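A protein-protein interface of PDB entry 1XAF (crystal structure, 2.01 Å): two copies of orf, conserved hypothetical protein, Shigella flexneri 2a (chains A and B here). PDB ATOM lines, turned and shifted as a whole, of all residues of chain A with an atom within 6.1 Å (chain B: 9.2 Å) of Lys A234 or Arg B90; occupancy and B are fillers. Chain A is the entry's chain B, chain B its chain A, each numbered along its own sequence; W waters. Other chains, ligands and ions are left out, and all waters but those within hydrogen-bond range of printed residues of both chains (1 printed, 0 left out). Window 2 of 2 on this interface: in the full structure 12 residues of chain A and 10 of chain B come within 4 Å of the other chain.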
ATOM      1  N   SER A 229      25.966  25.448  16.589  1.00  0.00           N
ATOM      2  CA  SER A 229      24.624  26.009  16.511  1.00  0.00           C
ATOM      3  C   SER A 229      23.829  25.581  17.735  1.00  0.00           C
ATOM      4  O   SER A 229      23.703  24.379  18.010  1.00  0.00           O
ATOM      5  CB  SER A 229      23.941  25.560  15.215  1.00  0.00           C
ATOM      6  OG  SER A 229      22.543  25.722  15.332  1.00  0.00           O
ATOM      7  N   TYR A 230      23.328  26.552  18.504  1.00  0.00           N
ATOM      8  CA  TYR A 230      22.581  26.260  19.709  1.00  0.00           C
ATOM      9  C   TYR A 230      21.261  25.500  19.407  1.00  0.00           C
ATOM     10  O   TYR A 230      20.851  24.539  20.119  1.00  0.00           O
ATOM     11  CB  TYR A 230      22.311  27.577  20.447  1.00  0.00           C
ATOM     12  CG  TYR A 230      21.454  27.425  21.654  1.00  0.00           C
ATOM     13  CD1 TYR A 230      21.988  26.934  22.846  1.00  0.00           C
ATOM     14  CD2 TYR A 230      20.114  27.789  21.630  1.00  0.00           C
ATOM     15  CE1 TYR A 230      21.202  26.787  23.975  1.00  0.00           C
ATOM     16  CE2 TYR A 230      19.299  27.625  22.766  1.00  0.00           C
ATOM     17  CZ  TYR A 230      19.869  27.121  23.930  1.00  0.00           C
ATOM     18  OH  TYR A 230      19.118  26.999  25.075  1.00  0.00           O
ATOM     19  N   ARG A 231      20.611  25.936  18.338  1.00  0.00           N
ATOM     20  CA  ARG A 231      19.369  25.312  17.903  1.00  0.00           C
ATOM     21  C   ARG A 231      19.609  23.853  17.466  1.00  0.00           C
ATOM     22  O   ARG A 231      18.833  22.949  17.804  1.00  0.00           O
ATOM     23  CB  ARG A 231      18.750  26.150  16.767  1.00  0.00           C
ATOM     24  CG  ARG A 231      17.585  25.493  16.053  1.00  0.00           C
ATOM     25  CD  ARG A 231      16.250  25.899  16.638  1.00  0.00           C
ATOM     26  NE  ARG A 231      15.090  25.102  16.143  1.00  0.00           N
ATOM     27  CZ  ARG A 231      14.707  24.967  14.863  1.00  0.00           C
ATOM     28  NH1 ARG A 231      15.406  25.525  13.878  1.00  0.00           N
ATOM     29  NH2 ARG A 231      13.626  24.245  14.563  1.00  0.00           N
ATOM     30  N   ARG A 232      20.674  23.625  16.719  1.00  0.00           N
ATOM     31  CA  ARG A 232      20.988  22.275  16.280  1.00  0.00           C
ATOM     32  C   ARG A 232      21.447  21.374  17.454  1.00  0.00           C
ATOM     33  O   ARG A 232      20.908  20.267  17.652  1.00  0.00           O
ATOM     34  CB  ARG A 232      22.040  22.338  15.161  1.00  0.00           C
ATOM     35  CG  ARG A 232      22.291  21.020  14.403  1.00  0.00           C
ATOM     36  CD  ARG A 232      23.509  21.136  13.470  1.00  0.00           C
ATOM     37  NE  ARG A 232      24.729  21.465  14.207  1.00  0.00           N
ATOM     38  CZ  ARG A 232      25.586  22.457  13.928  1.00  0.00           C
ATOM     39  NH1 ARG A 232      25.442  23.237  12.848  1.00  0.00           N
ATOM     40  NH2 ARG A 232      26.630  22.639  14.739  1.00  0.00           N
ATOM     41  N   ASP A 233      22.393  21.871  18.257  1.00  0.00           N
ATOM     42  CA  ASP A 233      23.133  21.023  19.211  1.00  0.00           C
ATOM     43  C   ASP A 233      22.639  21.054  20.662  1.00  0.00           C
ATOM     44  O   ASP A 233      22.914  20.113  21.430  1.00  0.00           O
ATOM     45  CB  ASP A 233      24.613  21.400  19.228  1.00  0.00           C
ATOM     46  CG  ASP A 233      25.259  21.405  17.855  1.00  0.00           C
ATOM     47  OD1 ASP A 233      25.026  20.452  17.089  1.00  0.00           O
ATOM     48  OD2 ASP A 233      26.045  22.358  17.554  1.00  0.00           O
ATOM     49  N   LYS A 234      21.974  22.143  21.051  1.00  0.00           N
ATOM     50  CA  LYS A 234      21.619  22.443  22.453  1.00  0.00           C
ATOM     51  C   LYS A 234      22.838  22.715  23.356  1.00  0.00           C
ATOM     52  O   LYS A 234      23.091  23.868  23.747  1.00  0.00           O
ATOM     53  CB  LYS A 234      20.691  21.374  23.064  1.00  0.00           C
ATOM     54  CG  LYS A 234      19.977  21.842  24.336  1.00  0.00           C
ATOM     55  CD  LYS A 234      20.796  21.618  25.653  1.00  0.00           C
ATOM     56  CE  LYS A 234      21.153  20.115  25.927  1.00  0.00           C
ATOM     57  NZ  LYS A 234      19.956  19.236  26.137  1.00  0.00           N
ATOM     58  N   THR A 235      23.597  21.664  23.650  1.00  0.00           N
ATOM     59  CA  THR A 235      24.859  21.769  24.369  1.00  0.00           C
ATOM     60  C   THR A 235      25.991  21.768  23.364  1.00  0.00           C
ATOM     61  O   THR A 235      26.182  20.812  22.632  1.00  0.00           O
ATOM     62  CB  THR A 235      25.066  20.595  25.348  1.00  0.00           C
ATOM     63  OG1 THR A 235      23.984  20.578  26.266  1.00  0.00           O
ATOM     64  CG2 THR A 235      26.353  20.798  26.169  1.00  0.00           C
ATOM     65  N   THR A 236      26.731  22.869  23.314  1.00  0.00           N
ATOM     66  CA  THR A 236      27.635  23.080  22.206  1.00  0.00           C
ATOM     67  C   THR A 236      28.559  24.252  22.515  1.00  0.00           C
ATOM     68  O   THR A 236      28.411  24.908  23.553  1.00  0.00           O
ATOM     69  CB  THR A 236      26.864  23.282  20.897  1.00  0.00           C
ATOM     70  OG1 THR A 236      27.730  23.008  19.778  1.00  0.00           O
ATOM     71  CG2 THR A 236      26.256  24.688  20.784  1.00  0.00           C
ATOM     72  N   ARG A 238      30.880  27.871  21.401  1.00  0.00           N
ATOM     73  CA  ARG A 238      30.559  29.221  20.941  1.00  0.00           C
ATOM     74  C   ARG A 238      31.640  29.763  20.036  1.00  0.00           C
ATOM     75  O   ARG A 238      32.832  29.512  20.254  1.00  0.00           O
ATOM     76  CB  ARG A 238      30.345  30.203  22.113  1.00  0.00           C
ATOM     77  CG  ARG A 238      29.179  29.863  23.082  1.00  0.00           C
ATOM     78  CD  ARG A 238      27.818  30.147  22.476  1.00  0.00           C
ATOM     79  NE  ARG A 238      26.745  29.817  23.411  1.00  0.00           N
ATOM     80  CZ  ARG A 238      26.266  28.588  23.630  1.00  0.00           C
ATOM     81  NH1 ARG A 238      26.739  27.538  22.973  1.00  0.00           N
ATOM     82  NH2 ARG A 238      25.299  28.407  24.527  1.00  0.00           N
ATOM     83  N   TRP B  69       8.987  12.385   9.393  1.00  0.00           N
ATOM     84  CA  TRP B  69      10.220  13.130   9.209  1.00  0.00           C
ATOM     85  C   TRP B  69      10.741  13.577  10.572  1.00  0.00           C
ATOM     86  O   TRP B  69       9.966  14.060  11.418  1.00  0.00           O
ATOM     87  CB  TRP B  69       9.981  14.332   8.317  1.00  0.00           C
ATOM     88  CG  TRP B  69       9.591  13.980   6.907  1.00  0.00           C
ATOM     89  CD1 TRP B  69       8.421  14.295   6.277  1.00  0.00           C
ATOM     90  CD2 TRP B  69      10.389  13.275   5.950  1.00  0.00           C
ATOM     91  NE1 TRP B  69       8.432  13.785   4.973  1.00  0.00           N
ATOM     92  CE2 TRP B  69       9.638  13.179   4.757  1.00  0.00           C
ATOM     93  CE3 TRP B  69      11.691  12.725   5.981  1.00  0.00           C
ATOM     94  CZ2 TRP B  69      10.132  12.544   3.614  1.00  0.00           C
ATOM     95  CZ3 TRP B  69      12.173  12.096   4.836  1.00  0.00           C
ATOM     96  CH2 TRP B  69      11.397  12.013   3.673  1.00  0.00           C
ATOM     97  N   LEU B  70      12.043  13.394  10.786  1.00  0.00           N
ATOM     98  CA  LEU B  70      12.705  13.835  12.008  1.00  0.00           C
ATOM     99  C   LEU B  70      13.284  15.218  11.773  1.00  0.00           C
ATOM    100  O   LEU B  70      13.441  15.664  10.639  1.00  0.00           O
ATOM    101  CB  LEU B  70      13.841  12.865  12.378  1.00  0.00           C
ATOM    102  CG  LEU B  70      13.484  11.385  12.541  1.00  0.00           C
ATOM    103  CD1 LEU B  70      14.759  10.553  12.742  1.00  0.00           C
ATOM    104  CD2 LEU B  70      12.480  11.183  13.691  1.00  0.00           C
ATOM    105  N   GLU B  71      13.591  15.909  12.854  1.00  0.00           N
ATOM    106  CA  GLU B  71      14.355  17.139  12.791  1.00  0.00           C
ATOM    107  C   GLU B  71      15.768  16.624  13.015  1.00  0.00           C
ATOM    108  O   GLU B  71      16.192  16.474  14.151  1.00  0.00           O
ATOM    109  CB  GLU B  71      13.908  18.055  13.952  1.00  0.00           C
ATOM    110  CG  GLU B  71      14.517  19.452  13.950  1.00  0.00           C
ATOM    111  CD  GLU B  71      14.318  20.145  15.312  1.00  0.00           C
ATOM    112  OE1 GLU B  71      13.162  20.135  15.833  1.00  0.00           O
ATOM    113  OE2 GLU B  71      15.319  20.672  15.859  1.00  0.00           O
ATOM    114  N   GLN B  72      16.484  16.309  11.936  1.00  0.00           N
ATOM    115  CA  GLN B  72      17.808  15.670  12.063  1.00  0.00           C
ATOM    116  C   GLN B  72      18.872  16.701  12.416  1.00  0.00           C
ATOM    117  O   GLN B  72      19.005  17.712  11.729  1.00  0.00           O
ATOM    118  CB  GLN B  72      18.207  14.974  10.753  1.00  0.00           C
ATOM    119  CG  GLN B  72      17.246  13.840  10.365  1.00  0.00           C
ATOM    120  CD  GLN B  72      17.439  13.337   8.938  1.00  0.00           C
ATOM    121  OE1 GLN B  72      18.381  13.725   8.219  1.00  0.00           O
ATOM    122  NE2 GLN B  72      16.546  12.489   8.520  1.00  0.00           N
ATOM    123  N   VAL B  73      19.651  16.412  13.448  1.00  0.00           N
ATOM    124  CA  VAL B  73      20.624  17.386  13.972  1.00  0.00           C
ATOM    125  C   VAL B  73      22.071  16.834  13.932  1.00  0.00           C
ATOM    126  O   VAL B  73      22.999  17.416  14.517  1.00  0.00           O
ATOM    127  CB  VAL B  73      20.198  17.872  15.397  1.00  0.00           C
ATOM    128  CG1 VAL B  73      18.951  18.722  15.351  1.00  0.00           C
ATOM    129  CG2 VAL B  73      19.969  16.720  16.330  1.00  0.00           C
ATOM    130  N   HIS B  74      22.260  15.711  13.230  1.00  0.00           N
ATOM    131  CA  HIS B  74      23.566  15.044  13.141  1.00  0.00           C
ATOM    132  C   HIS B  74      24.085  14.543  14.477  1.00  0.00           C
ATOM    133  O   HIS B  74      25.295  14.427  14.677  1.00  0.00           O
ATOM    134  CB  HIS B  74      24.605  15.925  12.431  1.00  0.00           C
ATOM    135  CG  HIS B  74      24.395  16.001  10.954  1.00  0.00           C
ATOM    136  ND1 HIS B  74      23.445  16.816  10.387  1.00  0.00           N
ATOM    137  CD2 HIS B  74      24.957  15.308   9.934  1.00  0.00           C
ATOM    138  CE1 HIS B  74      23.455  16.663   9.073  1.00  0.00           C
ATOM    139  NE2 HIS B  74      24.377  15.766   8.771  1.00  0.00           N
ATOM    140  N   GLY B  75      23.169  14.252  15.391  1.00  0.00           N
ATOM    141  CA  GLY B  75      23.540  13.599  16.632  1.00  0.00           C
ATOM    142  C   GLY B  75      23.300  12.108  16.597  1.00  0.00           C
ATOM    143  O   GLY B  75      23.366  11.483  15.536  1.00  0.00           O
ATOM    144  N   LYS B  76      22.996  11.543  17.763  1.00  0.00           N
ATOM    145  CA  LYS B  76      22.868  10.090  17.923  1.00  0.00           C
ATOM    146  C   LYS B  76      21.559   9.638  18.592  1.00  0.00           C
ATOM    147  O   LYS B  76      21.443   8.467  19.009  1.00  0.00           O
ATOM    148  CB  LYS B  76      24.037   9.565  18.759  1.00  0.00           C
ATOM    149  CG  LYS B  76      24.202  10.368  20.108  1.00  0.00           C
ATOM    150  CD  LYS B  76      25.192   9.749  21.059  1.00  0.00           C
ATOM    151  CE  LYS B  76      24.922   8.252  21.241  1.00  0.00           C
ATOM    152  NZ  LYS B  76      23.596   7.987  21.834  1.00  0.00           N
ATOM    153  N   ASP B  77      20.582  10.541  18.670  1.00  0.00           N
ATOM    154  CA  ASP B  77      19.323  10.285  19.348  1.00  0.00           C
ATOM    155  C   ASP B  77      18.338   9.498  18.464  1.00  0.00           C
ATOM    156  O   ASP B  77      18.259   9.725  17.265  1.00  0.00           O
ATOM    157  CB  ASP B  77      18.724  11.614  19.844  1.00  0.00           C
ATOM    158  CG  ASP B  77      19.496  12.189  21.058  1.00  0.00           C
ATOM    159  OD1 ASP B  77      20.230  11.408  21.724  1.00  0.00           O
ATOM    160  OD2 ASP B  77      19.376  13.413  21.334  1.00  0.00           O
ATOM    161  N   VAL B  78      17.645   8.542  19.081  1.00  0.00           N
ATOM    162  CA  VAL B  78      16.714   7.650  18.395  1.00  0.00           C
ATOM    163  C   VAL B  78      15.349   7.960  18.957  1.00  0.00           C
ATOM    164  O   VAL B  78      15.180   7.951  20.182  1.00  0.00           O
ATOM    165  CB  VAL B  78      17.048   6.131  18.634  1.00  0.00           C
ATOM    166  CG1 VAL B  78      16.075   5.195  17.854  1.00  0.00           C
ATOM    167  CG2 VAL B  78      18.456   5.814  18.256  1.00  0.00           C
ATOM    168  N   LEU B  79      14.395   8.274  18.077  1.00  0.00           N
ATOM    169  CA  LEU B  79      13.000   8.474  18.480  1.00  0.00           C
ATOM    170  C   LEU B  79      12.180   7.192  18.267  1.00  0.00           C
ATOM    171  O   LEU B  79      12.044   6.726  17.142  1.00  0.00           O
ATOM    172  CB  LEU B  79      12.377   9.627  17.703  1.00  0.00           C
ATOM    173  CG  LEU B  79      10.906   9.985  17.982  1.00  0.00           C
ATOM    174  CD1 LEU B  79      10.815  10.867  19.243  1.00  0.00           C
ATOM    175  CD2 LEU B  79      10.331  10.684  16.777  1.00  0.00           C
ATOM    176  N   LYS B  80      11.664   6.612  19.350  1.00  0.00           N
ATOM    177  CA  LYS B  80      10.750   5.485  19.242  1.00  0.00           C
ATOM    178  C   LYS B  80       9.371   6.012  18.857  1.00  0.00           C
ATOM    179  O   LYS B  80       8.786   6.827  19.572  1.00  0.00           O
ATOM    180  CB  LYS B  80      10.693   4.688  20.545  1.00  0.00           C
ATOM    181  CG  LYS B  80      11.990   3.925  20.915  1.00  0.00           C
ATOM    182  CD  LYS B  80      11.699   2.939  22.027  1.00  0.00           C
ATOM    183  CE  LYS B  80      12.963   2.245  22.541  1.00  0.00           C
ATOM    184  NZ  LYS B  80      12.657   1.318  23.699  1.00  0.00           N
ATOM    185  N   TYR B  86       4.547  13.711  20.262  1.00  0.00           N
ATOM    186  CA  TYR B  86       5.948  13.579  20.652  1.00  0.00           C
ATOM    187  C   TYR B  86       6.431  14.906  21.192  1.00  0.00           C
ATOM    188  O   TYR B  86       6.213  15.939  20.566  1.00  0.00           O
ATOM    189  CB  TYR B  86       6.818  13.235  19.430  1.00  0.00           C
ATOM    190  CG  TYR B  86       6.468  11.933  18.787  1.00  0.00           C
ATOM    191  CD1 TYR B  86       5.825  11.898  17.562  1.00  0.00           C
ATOM    192  CD2 TYR B  86       6.767  10.731  19.413  1.00  0.00           C
ATOM    193  CE1 TYR B  86       5.489  10.688  16.959  1.00  0.00           C
ATOM    194  CE2 TYR B  86       6.435   9.517  18.826  1.00  0.00           C
ATOM    195  CZ  TYR B  86       5.791   9.503  17.601  1.00  0.00           C
ATOM    196  OH  TYR B  86       5.447   8.300  17.023  1.00  0.00           O
ATOM    197  N   ALA B  87       7.128  14.867  22.327  1.00  0.00           N
ATOM    198  CA  ALA B  87       7.754  16.059  22.918  1.00  0.00           C
ATOM    199  C   ALA B  87       8.766  16.745  21.996  1.00  0.00           C
ATOM    200  O   ALA B  87       8.936  17.963  22.042  1.00  0.00           O
ATOM    201  CB  ALA B  87       8.407  15.702  24.252  1.00  0.00           C
ATOM    202  N   SER B  88       9.441  15.965  21.151  1.00  0.00           N
ATOM    203  CA  SER B  88      10.427  16.517  20.219  1.00  0.00           C
ATOM    204  C   SER B  88      10.751  15.501  19.124  1.00  0.00           C
ATOM    205  O   SER B  88      10.863  14.304  19.396  1.00  0.00           O
ATOM    206  CB  SER B  88      11.706  16.871  20.981  1.00  0.00           C
ATOM    207  OG  SER B  88      12.793  17.190  20.124  1.00  0.00           O
ATOM    208  N   LYS B  89      10.888  15.986  17.895  1.00  0.00           N
ATOM    209  CA  LYS B  89      11.362  15.155  16.776  1.00  0.00           C
ATOM    210  C   LYS B  89      12.850  15.362  16.465  1.00  0.00           C
ATOM    211  O   LYS B  89      13.316  14.960  15.384  1.00  0.00           O
ATOM    212  CB  LYS B  89      10.501  15.390  15.541  1.00  0.00           C
ATOM    213  CG  LYS B  89       9.113  14.801  15.722  1.00  0.00           C
ATOM    214  CD  LYS B  89       8.229  14.996  14.506  1.00  0.00           C
ATOM    215  CE  LYS B  89       7.035  14.049  14.640  1.00  0.00           C
ATOM    216  NZ  LYS B  89       5.792  14.613  14.058  1.00  0.00           N
ATOM    217  N   ARG B  90      13.573  15.984  17.405  1.00  0.00           N
ATOM    218  CA  ARG B  90      15.037  16.164  17.297  1.00  0.00           C
ATOM    219  C   ARG B  90      15.762  14.819  17.440  1.00  0.00           C
ATOM    220  O   ARG B  90      15.994  14.344  18.548  1.00  0.00           O
ATOM    221  CB  ARG B  90      15.564  17.148  18.361  1.00  0.00           C
ATOM    222  CG  ARG B  90      15.391  18.623  18.020  1.00  0.00           C
ATOM    223  CD  ARG B  90      15.996  19.607  19.079  1.00  0.00           C
ATOM    224  NE  ARG B  90      17.448  19.816  18.950  1.00  0.00           N
ATOM    225  CZ  ARG B  90      18.349  19.098  19.618  1.00  0.00           C
ATOM    226  NH1 ARG B  90      17.951  18.134  20.440  1.00  0.00           N
ATOM    227  NH2 ARG B  90      19.638  19.333  19.481  1.00  0.00           N
ATOM    228  N   ALA B  91      16.125  14.194  16.329  1.00  0.00           N
ATOM    229  CA  ALA B  91      16.667  12.854  16.397  1.00  0.00           C
ATOM    230  C   ALA B  91      17.306  12.521  15.077  1.00  0.00           C
ATOM    231  O   ALA B  91      17.018  13.152  14.049  1.00  0.00           O
ATOM    232  CB  ALA B  91      15.558  11.819  16.716  1.00  0.00           C
ATOM    233  N   ASP B  92      18.181  11.530  15.091  1.00  0.00           N
ATOM    234  CA  ASP B  92      18.792  11.140  13.822  1.00  0.00           C
ATOM    235  C   ASP B  92      18.506   9.690  13.458  1.00  0.00           C
ATOM    236  O   ASP B  92      19.025   9.197  12.471  1.00  0.00           O
ATOM    237  CB  ASP B  92      20.275  11.471  13.799  1.00  0.00           C
ATOM    238  CG  ASP B  92      20.536  12.993  13.631  1.00  0.00           C
ATOM    239  OD1 ASP B  92      20.741  13.454  12.473  1.00  0.00           O
ATOM    240  OD2 ASP B  92      20.526  13.725  14.663  1.00  0.00           O
ATOM    241  N   ALA B  93      17.693   9.023  14.263  1.00  0.00           N
ATOM    242  CA  ALA B  93      17.183   7.681  13.949  1.00  0.00           C
ATOM    243  C   ALA B  93      15.749   7.548  14.435  1.00  0.00           C
ATOM    244  O   ALA B  93      15.351   8.254  15.354  1.00  0.00           O
ATOM    245  CB  ALA B  93      18.031   6.620  14.615  1.00  0.00           C
ATOM    246  N   SER B  94      14.972   6.635  13.849  1.00  0.00           N
ATOM    247  CA  SER B  94      13.669   6.306  14.461  1.00  0.00           C
ATOM    248  C   SER B  94      13.469   4.795  14.483  1.00  0.00           C
ATOM    249  O   SER B  94      14.168   4.054  13.813  1.00  0.00           O
ATOM    250  CB  SER B  94      12.516   7.034  13.749  1.00  0.00           C
ATOM    251  OG  SER B  94      12.419   6.612  12.392  1.00  0.00           O
HETATM  252  O   HOH W   1      23.637  17.803  17.309  1.00  0.00           O
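NH2 of Arg B90 sits at hydrogen-bond distance from O of Arg A232 (2.4 Å).
The side-chain hydroxyl of Ser B88 is in hydrogen-bond range of the backbone NH of Arg B90 (3.1 Å).
OD2 of Asp A233 sits at hydrogen-bond distance from OG1 of Thr A236 (2.9 Å).
OE2 of Glu B71 is in salt-bridge range of NE of Arg B90.
OD2 of Asp A233 is in hydrogen-bond range of N of Ser A229 (3.2 Å).
OG of Ser A229 is in hydrogen-bond range of N of Arg A232 (3.1 Å).
NH2 of Arg A232 lies within salt-bridge range of OD2 of Asp A233 (2.9 Å).
Among the printed residues, pairs that only touch across the chains: Arg A232 with Val B73 (3.4 Å), Arg A231 with Arg B90 (3.6 Å), Asp A233 with Arg B90 (3.7 Å) and Lys A234 with Arg B90 (3.98 Å).
Of the printed residues of chain A, Arg B90 touches Arg A231 (3.6 Å), Arg A232 (2.4 Å), Asp A233 (3.7 Å) and Lys A234 (3.98 Å).
Printed residues of chain B within 4 Å of Asp A233: Arg B90.
Of the printed residues of chain A, Val B73 touches Arg A232 (3.4 Å).
Ser A229 touches none of the printed residues of chain B.
Ala B93 touches none of the printed residues of chain A.
Of the 9 printed residues of chain A, 4 touch a printed residue of chain B.
Of the 21 printed residues of chain B, 2 touch a printed residue of chain A.
Printed residues of chain B that touch a printed residue of chain A: Val B73 and Arg B90.
Among the printed residues, no Asp or Glu carboxylate lies within 4 Å of a Lys or Arg side-chain nitrogen of the other chain.
No position is printed for both chains.
Of the 5 pairs that touch across the chains among the printed residues, none has its exchanged pair printed and touching as well.
Water W1 bridges the backbone carbonyl oxygen of Val B73 (2.9 Å) and the side-chain carboxylate of Asp A233 (3.0 Å).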
